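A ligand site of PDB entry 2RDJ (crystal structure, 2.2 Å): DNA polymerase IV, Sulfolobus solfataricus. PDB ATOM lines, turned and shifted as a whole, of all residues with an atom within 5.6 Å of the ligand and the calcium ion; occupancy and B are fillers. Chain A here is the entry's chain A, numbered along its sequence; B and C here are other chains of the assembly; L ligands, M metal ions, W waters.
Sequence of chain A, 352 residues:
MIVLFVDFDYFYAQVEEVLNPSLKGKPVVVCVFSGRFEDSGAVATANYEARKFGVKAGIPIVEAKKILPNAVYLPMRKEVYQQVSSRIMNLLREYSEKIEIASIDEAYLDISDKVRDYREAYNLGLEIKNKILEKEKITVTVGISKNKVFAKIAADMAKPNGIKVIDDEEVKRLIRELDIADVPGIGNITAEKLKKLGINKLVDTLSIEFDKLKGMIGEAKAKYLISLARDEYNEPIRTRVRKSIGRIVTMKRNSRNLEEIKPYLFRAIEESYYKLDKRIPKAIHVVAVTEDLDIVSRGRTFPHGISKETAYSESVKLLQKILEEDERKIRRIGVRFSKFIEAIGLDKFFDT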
ATOM      1  N   ASP A   7     -18.160 -23.908 -24.039  1.00  0.00           N
ATOM      2  CA  ASP A   7     -18.108 -24.065 -22.566  1.00  0.00           C
ATOM      3  C   ASP A   7     -19.068 -25.203 -22.200  1.00  0.00           C
ATOM      4  O   ASP A   7     -20.291 -25.084 -22.402  1.00  0.00           O
ATOM      5  CB  ASP A   7     -18.509 -22.741 -21.878  1.00  0.00           C
ATOM      6  CG  ASP A   7     -18.280 -22.750 -20.359  1.00  0.00           C
ATOM      7  OD1 ASP A   7     -18.187 -23.816 -19.732  1.00  0.00           O
ATOM      8  OD2 ASP A   7     -18.193 -21.665 -19.769  1.00  0.00           O
ATOM      9  N   PHE A   8     -18.547 -26.313 -21.684  1.00  0.00           N
ATOM     10  CA  PHE A   8     -19.397 -27.474 -21.365  1.00  0.00           C
ATOM     11  C   PHE A   8     -20.274 -27.111 -20.171  1.00  0.00           C
ATOM     12  O   PHE A   8     -19.792 -26.515 -19.219  1.00  0.00           O
ATOM     13  CB  PHE A   8     -18.593 -28.745 -21.077  1.00  0.00           C
ATOM     14  CG  PHE A   8     -17.503 -29.055 -22.070  1.00  0.00           C
ATOM     15  CD1 PHE A   8     -17.530 -28.562 -23.367  1.00  0.00           C
ATOM     16  CD2 PHE A   8     -16.420 -29.852 -21.705  1.00  0.00           C
ATOM     17  CE1 PHE A   8     -16.480 -28.842 -24.258  1.00  0.00           C
ATOM     18  CE2 PHE A   8     -15.379 -30.160 -22.603  1.00  0.00           C
ATOM     19  CZ  PHE A   8     -15.426 -29.632 -23.885  1.00  0.00           C
ATOM     20  N   ASP A   9     -21.554 -27.471 -20.205  1.00  0.00           N
ATOM     21  CA  ASP A   9     -22.500 -27.027 -19.153  1.00  0.00           C
ATOM     22  C   ASP A   9     -22.322 -27.792 -17.830  1.00  0.00           C
ATOM     23  O   ASP A   9     -22.197 -29.007 -17.840  1.00  0.00           O
ATOM     24  CB  ASP A   9     -23.937 -27.151 -19.617  1.00  0.00           C
ATOM     25  CG  ASP A   9     -24.242 -26.290 -20.823  1.00  0.00           C
ATOM     26  OD1 ASP A   9     -23.771 -25.144 -20.866  1.00  0.00           O
ATOM     27  OD2 ASP A   9     -24.914 -26.790 -21.743  1.00  0.00           O
ATOM     28  N   TYR A  10     -22.339 -27.054 -16.724  1.00  0.00           N
ATOM     29  CA  TYR A  10     -22.157 -27.591 -15.362  1.00  0.00           C
ATOM     30  C   TYR A  10     -21.313 -28.892 -15.389  1.00  0.00           C
ATOM     31  O   TYR A  10     -21.751 -29.950 -14.931  1.00  0.00           O
ATOM     32  CB  TYR A  10     -23.522 -27.706 -14.645  1.00  0.00           C
ATOM     33  CG  TYR A  10     -24.522 -28.634 -15.343  1.00  0.00           C
ATOM     34  CD1 TYR A  10     -24.787 -29.929 -14.852  1.00  0.00           C
ATOM     35  CD2 TYR A  10     -25.202 -28.233 -16.521  1.00  0.00           C
ATOM     36  CE1 TYR A  10     -25.684 -30.766 -15.486  1.00  0.00           C
ATOM     37  CE2 TYR A  10     -26.089 -29.087 -17.184  1.00  0.00           C
ATOM     38  CZ  TYR A  10     -26.328 -30.356 -16.657  1.00  0.00           C
ATOM     39  OH  TYR A  10     -27.246 -31.213 -17.272  1.00  0.00           O
ATOM     40  N   PHE A  11     -20.095 -28.803 -15.907  1.00  0.00           N
ATOM     41  CA  PHE A  11     -19.442 -30.011 -16.476  1.00  0.00           C
ATOM     42  C   PHE A  11     -19.350 -31.278 -15.572  1.00  0.00           C
ATOM     43  O   PHE A  11     -19.885 -32.327 -15.912  1.00  0.00           O
ATOM     44  CB  PHE A  11     -18.084 -29.664 -17.119  1.00  0.00           C
ATOM     45  CG  PHE A  11     -17.466 -30.826 -17.870  1.00  0.00           C
ATOM     46  CD1 PHE A  11     -18.168 -31.448 -18.907  1.00  0.00           C
ATOM     47  CD2 PHE A  11     -16.211 -31.279 -17.544  1.00  0.00           C
ATOM     48  CE1 PHE A  11     -17.606 -32.508 -19.605  1.00  0.00           C
ATOM     49  CE2 PHE A  11     -15.653 -32.345 -18.211  1.00  0.00           C
ATOM     50  CZ  PHE A  11     -16.355 -32.967 -19.249  1.00  0.00           C
ATOM     51  N   TYR A  12     -18.673 -31.192 -14.432  1.00  0.00           N
ATOM     52  CA  TYR A  12     -18.505 -32.363 -13.575  1.00  0.00           C
ATOM     53  C   TYR A  12     -19.836 -32.979 -13.223  1.00  0.00           C
ATOM     54  O   TYR A  12     -19.946 -34.180 -13.208  1.00  0.00           O
ATOM     55  CB  TYR A  12     -17.773 -32.057 -12.270  1.00  0.00           C
ATOM     56  CG  TYR A  12     -16.419 -31.392 -12.377  1.00  0.00           C
ATOM     57  CD1 TYR A  12     -15.694 -31.382 -13.576  1.00  0.00           C
ATOM     58  CD2 TYR A  12     -15.850 -30.779 -11.265  1.00  0.00           C
ATOM     59  CE1 TYR A  12     -14.456 -30.785 -13.651  1.00  0.00           C
ATOM     60  CE2 TYR A  12     -14.609 -30.173 -11.338  1.00  0.00           C
ATOM     61  CZ  TYR A  12     -13.916 -30.177 -12.526  1.00  0.00           C
ATOM     62  OH  TYR A  12     -12.669 -29.568 -12.578  1.00  0.00           O
ATOM     63  N   VAL A  43     -17.700 -27.416  -2.271  1.00  0.00           N
ATOM     64  CA  VAL A  43     -18.402 -27.820  -3.484  1.00  0.00           C
ATOM     65  C   VAL A  43     -17.532 -27.428  -4.664  1.00  0.00           C
ATOM     66  O   VAL A  43     -17.085 -26.283  -4.757  1.00  0.00           O
ATOM     67  CB  VAL A  43     -19.811 -27.134  -3.603  1.00  0.00           C
ATOM     68  CG1 VAL A  43     -20.450 -27.406  -4.989  1.00  0.00           C
ATOM     69  CG2 VAL A  43     -20.740 -27.638  -2.501  1.00  0.00           C
ATOM     70  N   ALA A  44     -17.257 -28.382  -5.544  1.00  0.00           N
ATOM     71  CA  ALA A  44     -16.533 -28.136  -6.775  1.00  0.00           C
ATOM     72  C   ALA A  44     -17.468 -27.565  -7.833  1.00  0.00           C
ATOM     73  O   ALA A  44     -17.119 -26.596  -8.505  1.00  0.00           O
ATOM     74  CB  ALA A  44     -15.847 -29.432  -7.293  1.00  0.00           C
ATOM     75  N   THR A  45     -18.643 -28.174  -7.996  1.00  0.00           N
ATOM     76  CA  THR A  45     -19.689 -27.593  -8.829  1.00  0.00           C
ATOM     77  C   THR A  45     -21.042 -28.271  -8.545  1.00  0.00           C
ATOM     78  O   THR A  45     -21.128 -29.322  -7.924  1.00  0.00           O
ATOM     79  CB  THR A  45     -19.356 -27.707 -10.359  1.00  0.00           C
ATOM     80  OG1 THR A  45     -20.129 -26.713 -11.079  1.00  0.00           O
ATOM     81  CG2 THR A  45     -19.723 -29.074 -10.892  1.00  0.00           C
ATOM     82  N   ALA A  46     -22.108 -27.681  -9.053  1.00  0.00           N
ATOM     83  CA  ALA A  46     -23.417 -28.234  -8.845  1.00  0.00           C
ATOM     84  C   ALA A  46     -24.238 -28.033 -10.124  1.00  0.00           C
ATOM     85  O   ALA A  46     -23.937 -27.151 -10.900  1.00  0.00           O
ATOM     86  CB  ALA A  46     -24.072 -27.557  -7.634  1.00  0.00           C
ATOM     87  N   TYR A  48     -27.803 -27.191 -12.330  1.00  0.00           N
ATOM     88  CA  TYR A  48     -28.665 -26.031 -12.238  1.00  0.00           C
ATOM     89  C   TYR A  48     -29.839 -26.197 -11.263  1.00  0.00           C
ATOM     90  O   TYR A  48     -30.372 -25.220 -10.745  1.00  0.00           O
ATOM     91  CB  TYR A  48     -29.062 -25.544 -13.641  1.00  0.00           C
ATOM     92  CG  TYR A  48     -27.896 -24.808 -14.298  1.00  0.00           C
ATOM     93  CD1 TYR A  48     -26.922 -25.504 -15.030  1.00  0.00           C
ATOM     94  CD2 TYR A  48     -27.742 -23.438 -14.141  1.00  0.00           C
ATOM     95  CE1 TYR A  48     -25.860 -24.842 -15.606  1.00  0.00           C
ATOM     96  CE2 TYR A  48     -26.692 -22.771 -14.724  1.00  0.00           C
ATOM     97  CZ  TYR A  48     -25.748 -23.469 -15.451  1.00  0.00           C
ATOM     98  OH  TYR A  48     -24.709 -22.766 -16.032  1.00  0.00           O
ATOM     99  N   ARG A  51     -28.143 -25.209  -8.087  1.00  0.00           N
ATOM    100  CA  ARG A  51     -27.822 -23.765  -8.095  1.00  0.00           C
ATOM    101  C   ARG A  51     -29.071 -22.912  -7.925  1.00  0.00           C
ATOM    102  O   ARG A  51     -29.001 -21.767  -7.461  1.00  0.00           O
ATOM    103  CB  ARG A  51     -27.162 -23.344  -9.420  1.00  0.00           C
ATOM    104  CG  ARG A  51     -25.749 -23.808  -9.626  1.00  0.00           C
ATOM    105  CD  ARG A  51     -25.244 -23.358 -10.999  1.00  0.00           C
ATOM    106  NE  ARG A  51     -24.293 -24.344 -11.498  1.00  0.00           N
ATOM    107  CZ  ARG A  51     -23.336 -24.107 -12.391  1.00  0.00           C
ATOM    108  NH1 ARG A  51     -23.197 -22.890 -12.927  1.00  0.00           N
ATOM    109  NH2 ARG A  51     -22.485 -25.089 -12.744  1.00  0.00           N
ATOM    110  N   ALA A  57     -20.606 -23.816  -6.822  1.00  0.00           N
ATOM    111  CA  ALA A  57     -19.142 -23.976  -6.718  1.00  0.00           C
ATOM    112  C   ALA A  57     -18.560 -23.093  -5.620  1.00  0.00           C
ATOM    113  O   ALA A  57     -18.880 -21.891  -5.526  1.00  0.00           O
ATOM    114  CB  ALA A  57     -18.470 -23.666  -8.048  1.00  0.00           C
ATOM    115  N   GLY A  58     -17.724 -23.675  -4.771  1.00  0.00           N
ATOM    116  CA  GLY A  58     -16.983 -22.862  -3.809  1.00  0.00           C
ATOM    117  C   GLY A  58     -17.556 -22.767  -2.412  1.00  0.00           C
ATOM    118  O   GLY A  58     -16.870 -22.308  -1.518  1.00  0.00           O
ATOM    119  N   ILE A 104     -10.429 -27.569 -18.568  1.00  0.00           N
ATOM    120  CA  ILE A 104     -11.080 -28.860 -18.750  1.00  0.00           C
ATOM    121  C   ILE A 104     -12.385 -28.786 -19.558  1.00  0.00           C
ATOM    122  O   ILE A 104     -12.836 -29.784 -20.120  1.00  0.00           O
ATOM    123  CB  ILE A 104     -11.358 -29.558 -17.368  1.00  0.00           C
ATOM    124  CG1 ILE A 104     -11.777 -31.005 -17.609  1.00  0.00           C
ATOM    125  CG2 ILE A 104     -12.400 -28.769 -16.531  1.00  0.00           C
ATOM    126  CD1 ILE A 104     -11.384 -31.953 -16.509  1.00  0.00           C
ATOM    127  N   ASP A 105     -12.999 -27.609 -19.590  1.00  0.00           N
ATOM    128  CA  ASP A 105     -14.308 -27.512 -20.188  1.00  0.00           C
ATOM    129  C   ASP A 105     -14.517 -26.283 -21.052  1.00  0.00           C
ATOM    130  O   ASP A 105     -15.653 -25.914 -21.329  1.00  0.00           O
ATOM    131  CB  ASP A 105     -15.404 -27.629 -19.126  1.00  0.00           C
ATOM    132  CG  ASP A 105     -15.483 -26.432 -18.216  1.00  0.00           C
ATOM    133  OD1 ASP A 105     -14.437 -25.823 -17.892  1.00  0.00           O
ATOM    134  OD2 ASP A 105     -16.601 -26.106 -17.798  1.00  0.00           O
ATOM    135  N   LYS A 159     -25.607 -19.512 -21.570  1.00  0.00           N
ATOM    136  CA  LYS A 159     -25.575 -20.758 -20.797  1.00  0.00           C
ATOM    137  C   LYS A 159     -26.700 -20.910 -19.773  1.00  0.00           C
ATOM    138  O   LYS A 159     -27.136 -19.917 -19.182  1.00  0.00           O
ATOM    139  CB  LYS A 159     -24.219 -20.952 -20.132  1.00  0.00           C
ATOM    140  CG  LYS A 159     -23.842 -19.949 -19.076  1.00  0.00           C
ATOM    141  CD  LYS A 159     -22.628 -20.455 -18.239  1.00  0.00           C
ATOM    142  CE  LYS A 159     -21.328 -20.661 -19.098  1.00  0.00           C
ATOM    143  NZ  LYS A 159     -20.115 -20.742 -18.191  1.00  0.00           N
ATOM    144  P    DT B   2     -10.931 -25.726   1.913  1.00  0.00           P
ATOM    145  OP1  DT B   2     -11.051 -26.610   3.146  1.00  0.00           O
ATOM    146  OP2  DT B   2      -9.666 -25.021   1.548  1.00  0.00           O
ATOM    147  O5'  DT B   2     -11.380 -26.573   0.633  1.00  0.00           O
ATOM    148  C5'  DT B   2     -11.591 -27.968   0.775  1.00  0.00           C
ATOM    149  C4'  DT B   2     -11.009 -28.616  -0.457  1.00  0.00           C
ATOM    150  O4'  DT B   2     -11.722 -28.215  -1.639  1.00  0.00           O
ATOM    151  C3'  DT B   2      -9.535 -28.330  -0.714  1.00  0.00           C
ATOM    152  O3'  DT B   2      -9.033 -29.601  -1.021  1.00  0.00           O
ATOM    153  C2'  DT B   2      -9.506 -27.356  -1.891  1.00  0.00           C
ATOM    154  C1'  DT B   2     -10.845 -27.645  -2.594  1.00  0.00           C
ATOM    155  N1   DT B   2     -11.580 -26.470  -3.179  1.00  0.00           N
ATOM    156  C2   DT B   2     -11.967 -26.539  -4.493  1.00  0.00           C
ATOM    157  O2   DT B   2     -11.725 -27.505  -5.200  1.00  0.00           O
ATOM    158  N3   DT B   2     -12.657 -25.432  -4.958  1.00  0.00           N
ATOM    159  C4   DT B   2     -12.974 -24.317  -4.233  1.00  0.00           C
ATOM    160  O4   DT B   2     -13.586 -23.379  -4.724  1.00  0.00           O
ATOM    161  C5   DT B   2     -12.537 -24.293  -2.847  1.00  0.00           C
ATOM    162  C7   DT B   2     -12.841 -23.099  -1.983  1.00  0.00           C
ATOM    163  C6   DT B   2     -11.870 -25.360  -2.386  1.00  0.00           C
ATOM    164  P    DA B   3      -7.481 -29.892  -1.271  1.00  0.00           P
ATOM    165  OP1  DA B   3      -7.278 -31.304  -0.910  1.00  0.00           O
ATOM    166  OP2  DA B   3      -6.645 -28.788  -0.723  1.00  0.00           O
ATOM    167  O5'  DA B   3      -7.449 -29.742  -2.867  1.00  0.00           O
ATOM    168  C5'  DA B   3      -8.067 -30.689  -3.713  1.00  0.00           C
ATOM    169  C4'  DA B   3      -7.755 -30.342  -5.158  1.00  0.00           C
ATOM    170  O4'  DA B   3      -8.502 -29.175  -5.574  1.00  0.00           O
ATOM    171  C3'  DA B   3      -6.279 -30.001  -5.420  1.00  0.00           C
ATOM    172  O3'  DA B   3      -5.976 -30.716  -6.591  1.00  0.00           O
ATOM    173  C2'  DA B   3      -6.270 -28.504  -5.622  1.00  0.00           C
ATOM    174  C1'  DA B   3      -7.651 -28.279  -6.252  1.00  0.00           C
ATOM    175  N9   DA B   3      -8.245 -26.947  -6.112  1.00  0.00           N
ATOM    176  C8   DA B   3      -8.334 -26.181  -4.984  1.00  0.00           C
ATOM    177  N7   DA B   3      -8.947 -25.036  -5.186  1.00  0.00           N
ATOM    178  C5   DA B   3      -9.288 -25.056  -6.534  1.00  0.00           C
ATOM    179  C6   DA B   3      -9.970 -24.140  -7.359  1.00  0.00           C
ATOM    180  N6   DA B   3     -10.425 -22.954  -6.949  1.00  0.00           N
ATOM    181  N1   DA B   3     -10.154 -24.473  -8.653  1.00  0.00           N
ATOM    182  C2   DA B   3      -9.672 -25.663  -9.080  1.00  0.00           C
ATOM    183  N3   DA B   3      -9.025 -26.620  -8.390  1.00  0.00           N
ATOM    184  C4   DA B   3      -8.863 -26.234  -7.107  1.00  0.00           C
ATOM    185  P    DT C  14     -14.844 -19.146 -15.439  1.00  0.00           P
ATOM    186  OP1  DT C  14     -15.787 -18.926 -16.552  1.00  0.00           O
ATOM    187  OP2  DT C  14     -15.263 -18.747 -14.070  1.00  0.00           O
ATOM    188  O5'  DT C  14     -14.465 -20.701 -15.367  1.00  0.00           O
ATOM    189  C5'  DT C  14     -13.788 -21.331 -16.451  1.00  0.00           C
ATOM    190  C4'  DT C  14     -13.161 -22.675 -16.080  1.00  0.00           C
ATOM    191  O4'  DT C  14     -11.975 -22.518 -15.221  1.00  0.00           O
ATOM    192  C3'  DT C  14     -14.065 -23.606 -15.286  1.00  0.00           C
ATOM    193  O3'  DT C  14     -15.163 -24.198 -16.074  1.00  0.00           O
ATOM    194  C2'  DT C  14     -13.016 -24.575 -14.756  1.00  0.00           C
ATOM    195  C1'  DT C  14     -11.896 -23.617 -14.325  1.00  0.00           C
ATOM    196  N1   DT C  14     -11.922 -23.123 -12.890  1.00  0.00           N
ATOM    197  C2   DT C  14     -11.171 -23.769 -11.897  1.00  0.00           C
ATOM    198  O2   DT C  14     -10.471 -24.755 -12.087  1.00  0.00           O
ATOM    199  N3   DT C  14     -11.259 -23.209 -10.643  1.00  0.00           N
ATOM    200  C4   DT C  14     -12.028 -22.098 -10.265  1.00  0.00           C
ATOM    201  O4   DT C  14     -12.022 -21.695  -9.108  1.00  0.00           O
ATOM    202  C5   DT C  14     -12.778 -21.470 -11.316  1.00  0.00           C
ATOM    203  C7   DT C  14     -13.599 -20.223 -11.066  1.00  0.00           C
ATOM    204  C6   DT C  14     -12.690 -22.000 -12.561  1.00  0.00           C
HETATM  205  P1  LIG L   1     -19.580 -25.380 -14.638  1.00  0.00           P
HETATM  206  O1  LIG L   1     -19.358 -26.110 -15.948  1.00  0.00           O
HETATM  207  O2  LIG L   1     -20.536 -24.199 -14.640  1.00  0.00           O
HETATM  208  O3  LIG L   1     -19.722 -26.325 -13.474  1.00  0.00           O
HETATM  209  O4  LIG L   1     -18.123 -24.770 -14.494  1.00  0.00           O
HETATM  210  C1  LIG L   1     -17.947 -23.409 -14.162  1.00  0.00           C
HETATM  211  C2  LIG L   1     -17.868 -23.353 -12.670  1.00  0.00           C
HETATM  212  O5  LIG L   1     -17.123 -24.487 -12.170  1.00  0.00           O
HETATM  213  C3  LIG L   1     -17.048 -22.133 -12.423  1.00  0.00           C
HETATM  214  O6  LIG L   1     -17.383 -21.653 -11.097  1.00  0.00           O
HETATM  215  C4  LIG L   1     -15.646 -22.722 -12.549  1.00  0.00           C
HETATM  216  C5  LIG L   1     -15.707 -24.226 -12.297  1.00  0.00           C
HETATM  217  N1  LIG L   1     -14.968 -24.632 -11.089  1.00  0.00           N
HETATM  218  C6  LIG L   1     -14.121 -25.794 -11.072  1.00  0.00           C
HETATM  219  O7  LIG L   1     -13.945 -26.509 -12.083  1.00  0.00           O
HETATM  220  N2  LIG L   1     -13.443 -26.146  -9.953  1.00  0.00           N
HETATM  221  C7  LIG L   1     -13.573 -25.425  -8.811  1.00  0.00           C
HETATM  222  O8  LIG L   1     -12.969 -25.776  -7.774  1.00  0.00           O
HETATM  223  C8  LIG L   1     -14.458 -24.239  -8.792  1.00  0.00           C
HETATM  224  C9  LIG L   1     -14.634 -23.389  -7.548  1.00  0.00           C
HETATM  225  C10 LIG L   1     -15.108 -23.891  -9.971  1.00  0.00           C
HETATM  226 CA    CA M   1     -18.652 -25.049 -17.846  1.00  0.00          CA
HETATM  227  O   HOH W   1     -17.772 -28.413 -13.710  1.00  0.00           O
HETATM  228  O   HOH W   2     -20.581 -23.732 -18.004  1.00  0.00           O
HETATM  229  O   HOH W   3     -17.403 -23.258 -17.113  1.00  0.00           O
HETATM  230  O   HOH W   4     -19.909 -21.704 -15.245  1.00  0.00           O
HETATM  231  O   HOH W   5     -20.542 -21.844 -10.627  1.00  0.00           O
HETATM  232  O   HOH W   6     -15.558 -27.322 -14.613  1.00  0.00           O
HETATM  233  O   HOH W   7     -11.744 -28.495 -10.290  1.00  0.00           O
HETATM  234  O   HOH W   8     -12.317 -28.830  -7.764  1.00  0.00           O
HETATM  235  O   HOH W   9     -22.473 -24.305 -16.402  1.00  0.00           O
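An oxygen (O3) of the ligand sits at hydrogen-bond distance from the backbone NH (N) of Phe 11 (3.5 Å). OH of Tyr 12 lies within hydrogen-bond range of O7 of the ligand (3.4 Å). An oxygen (O2) of the ligand lies within salt-bridge range of the guanidinium group of Arg 51 (2.9 Å). The backbone NH (N) of Tyr 10 lies close to an oxygen (O1) of the ligand (3.2 Å). The side-chain hydroxyl (OG1) of Thr 45 sits at hydrogen-bond distance from an oxygen (O3) of the ligand, at 2.5 Å.
Water W2 lies within hydrogen-bond range of NZ of Lys 159 (3.0 Å) and O2 of the ligand (3.4 Å). Water W9 lies within hydrogen-bond range of O2 of the ligand (2.6 Å), OH of Tyr 48 (2.7 Å) and N of Tyr 10 (2.8 Å). Water W1 lies within hydrogen-bond range of an oxygen (O3) of the ligand (2.9 Å), the backbone NH (N) of Tyr 12 (3.0 Å) and the backbone NH (N) of Phe 11 (3.2 Å). Water W7 bridges OH of Tyr 12 (2.7 Å) and N2 of the ligand (2.9 Å). Water W6 bridges O7 of the ligand (3.1 Å) and O3' of DT 14 of chain C (3.5 Å). Water W8 bridges O2 of DT 2 of chain B and O8 of the ligand.
An oxygen (O8) of the ligand lies close to N3 of DT 2 of chain B, at 2.9 Å. N1 of DA 3 of chain B sits close to an oxygen (O8) of the ligand. O3' of DT 14 of chain C lies close to O4 of the ligand. Asp 9 touches the ligand. Ala 44 touches the ligand. Ala 57 touches the ligand. Hydrophobic or aromatic side chains that line the ligand: Phe 11, Tyr 12 and Ala 57. Of the 20 residues printed, 13 come within 4 Å of the ligand. The nearest printed residue that does not touch the ligand is Gly 58 (4.2 Å).
NE of Arg 51 lies within hydrogen-bond range of O of Ala 46 (2.9 Å). The side-chain carboxylate of Asp 105 sits close to O3' of DT 14 of chain C (2.5 Å). OG1 of Thr 45 sits at hydrogen-bond distance from NH2 of Arg 51. OD2 of Asp 7 lies within salt-bridge range of NZ of Lys 159 (2.7 Å). NH1 of Arg 51 is in hydrogen-bond range of OH of Tyr 48 (3.5 Å). N3 of DT 14 of chain C sits close to N1 of DA 3 of chain B, 2.6 Å away.
The calcium ion is bound by O1 of the ligand (2.3 Å), OD1 of Asp 7 (2.3 Å), water W3 (2.3 Å), OD2 of Asp 105 (2.3 Å), O of Phe 8 (2.3 Å) and water W2 (2.3 Å). The calcium ion has six donor atoms within binding distance.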
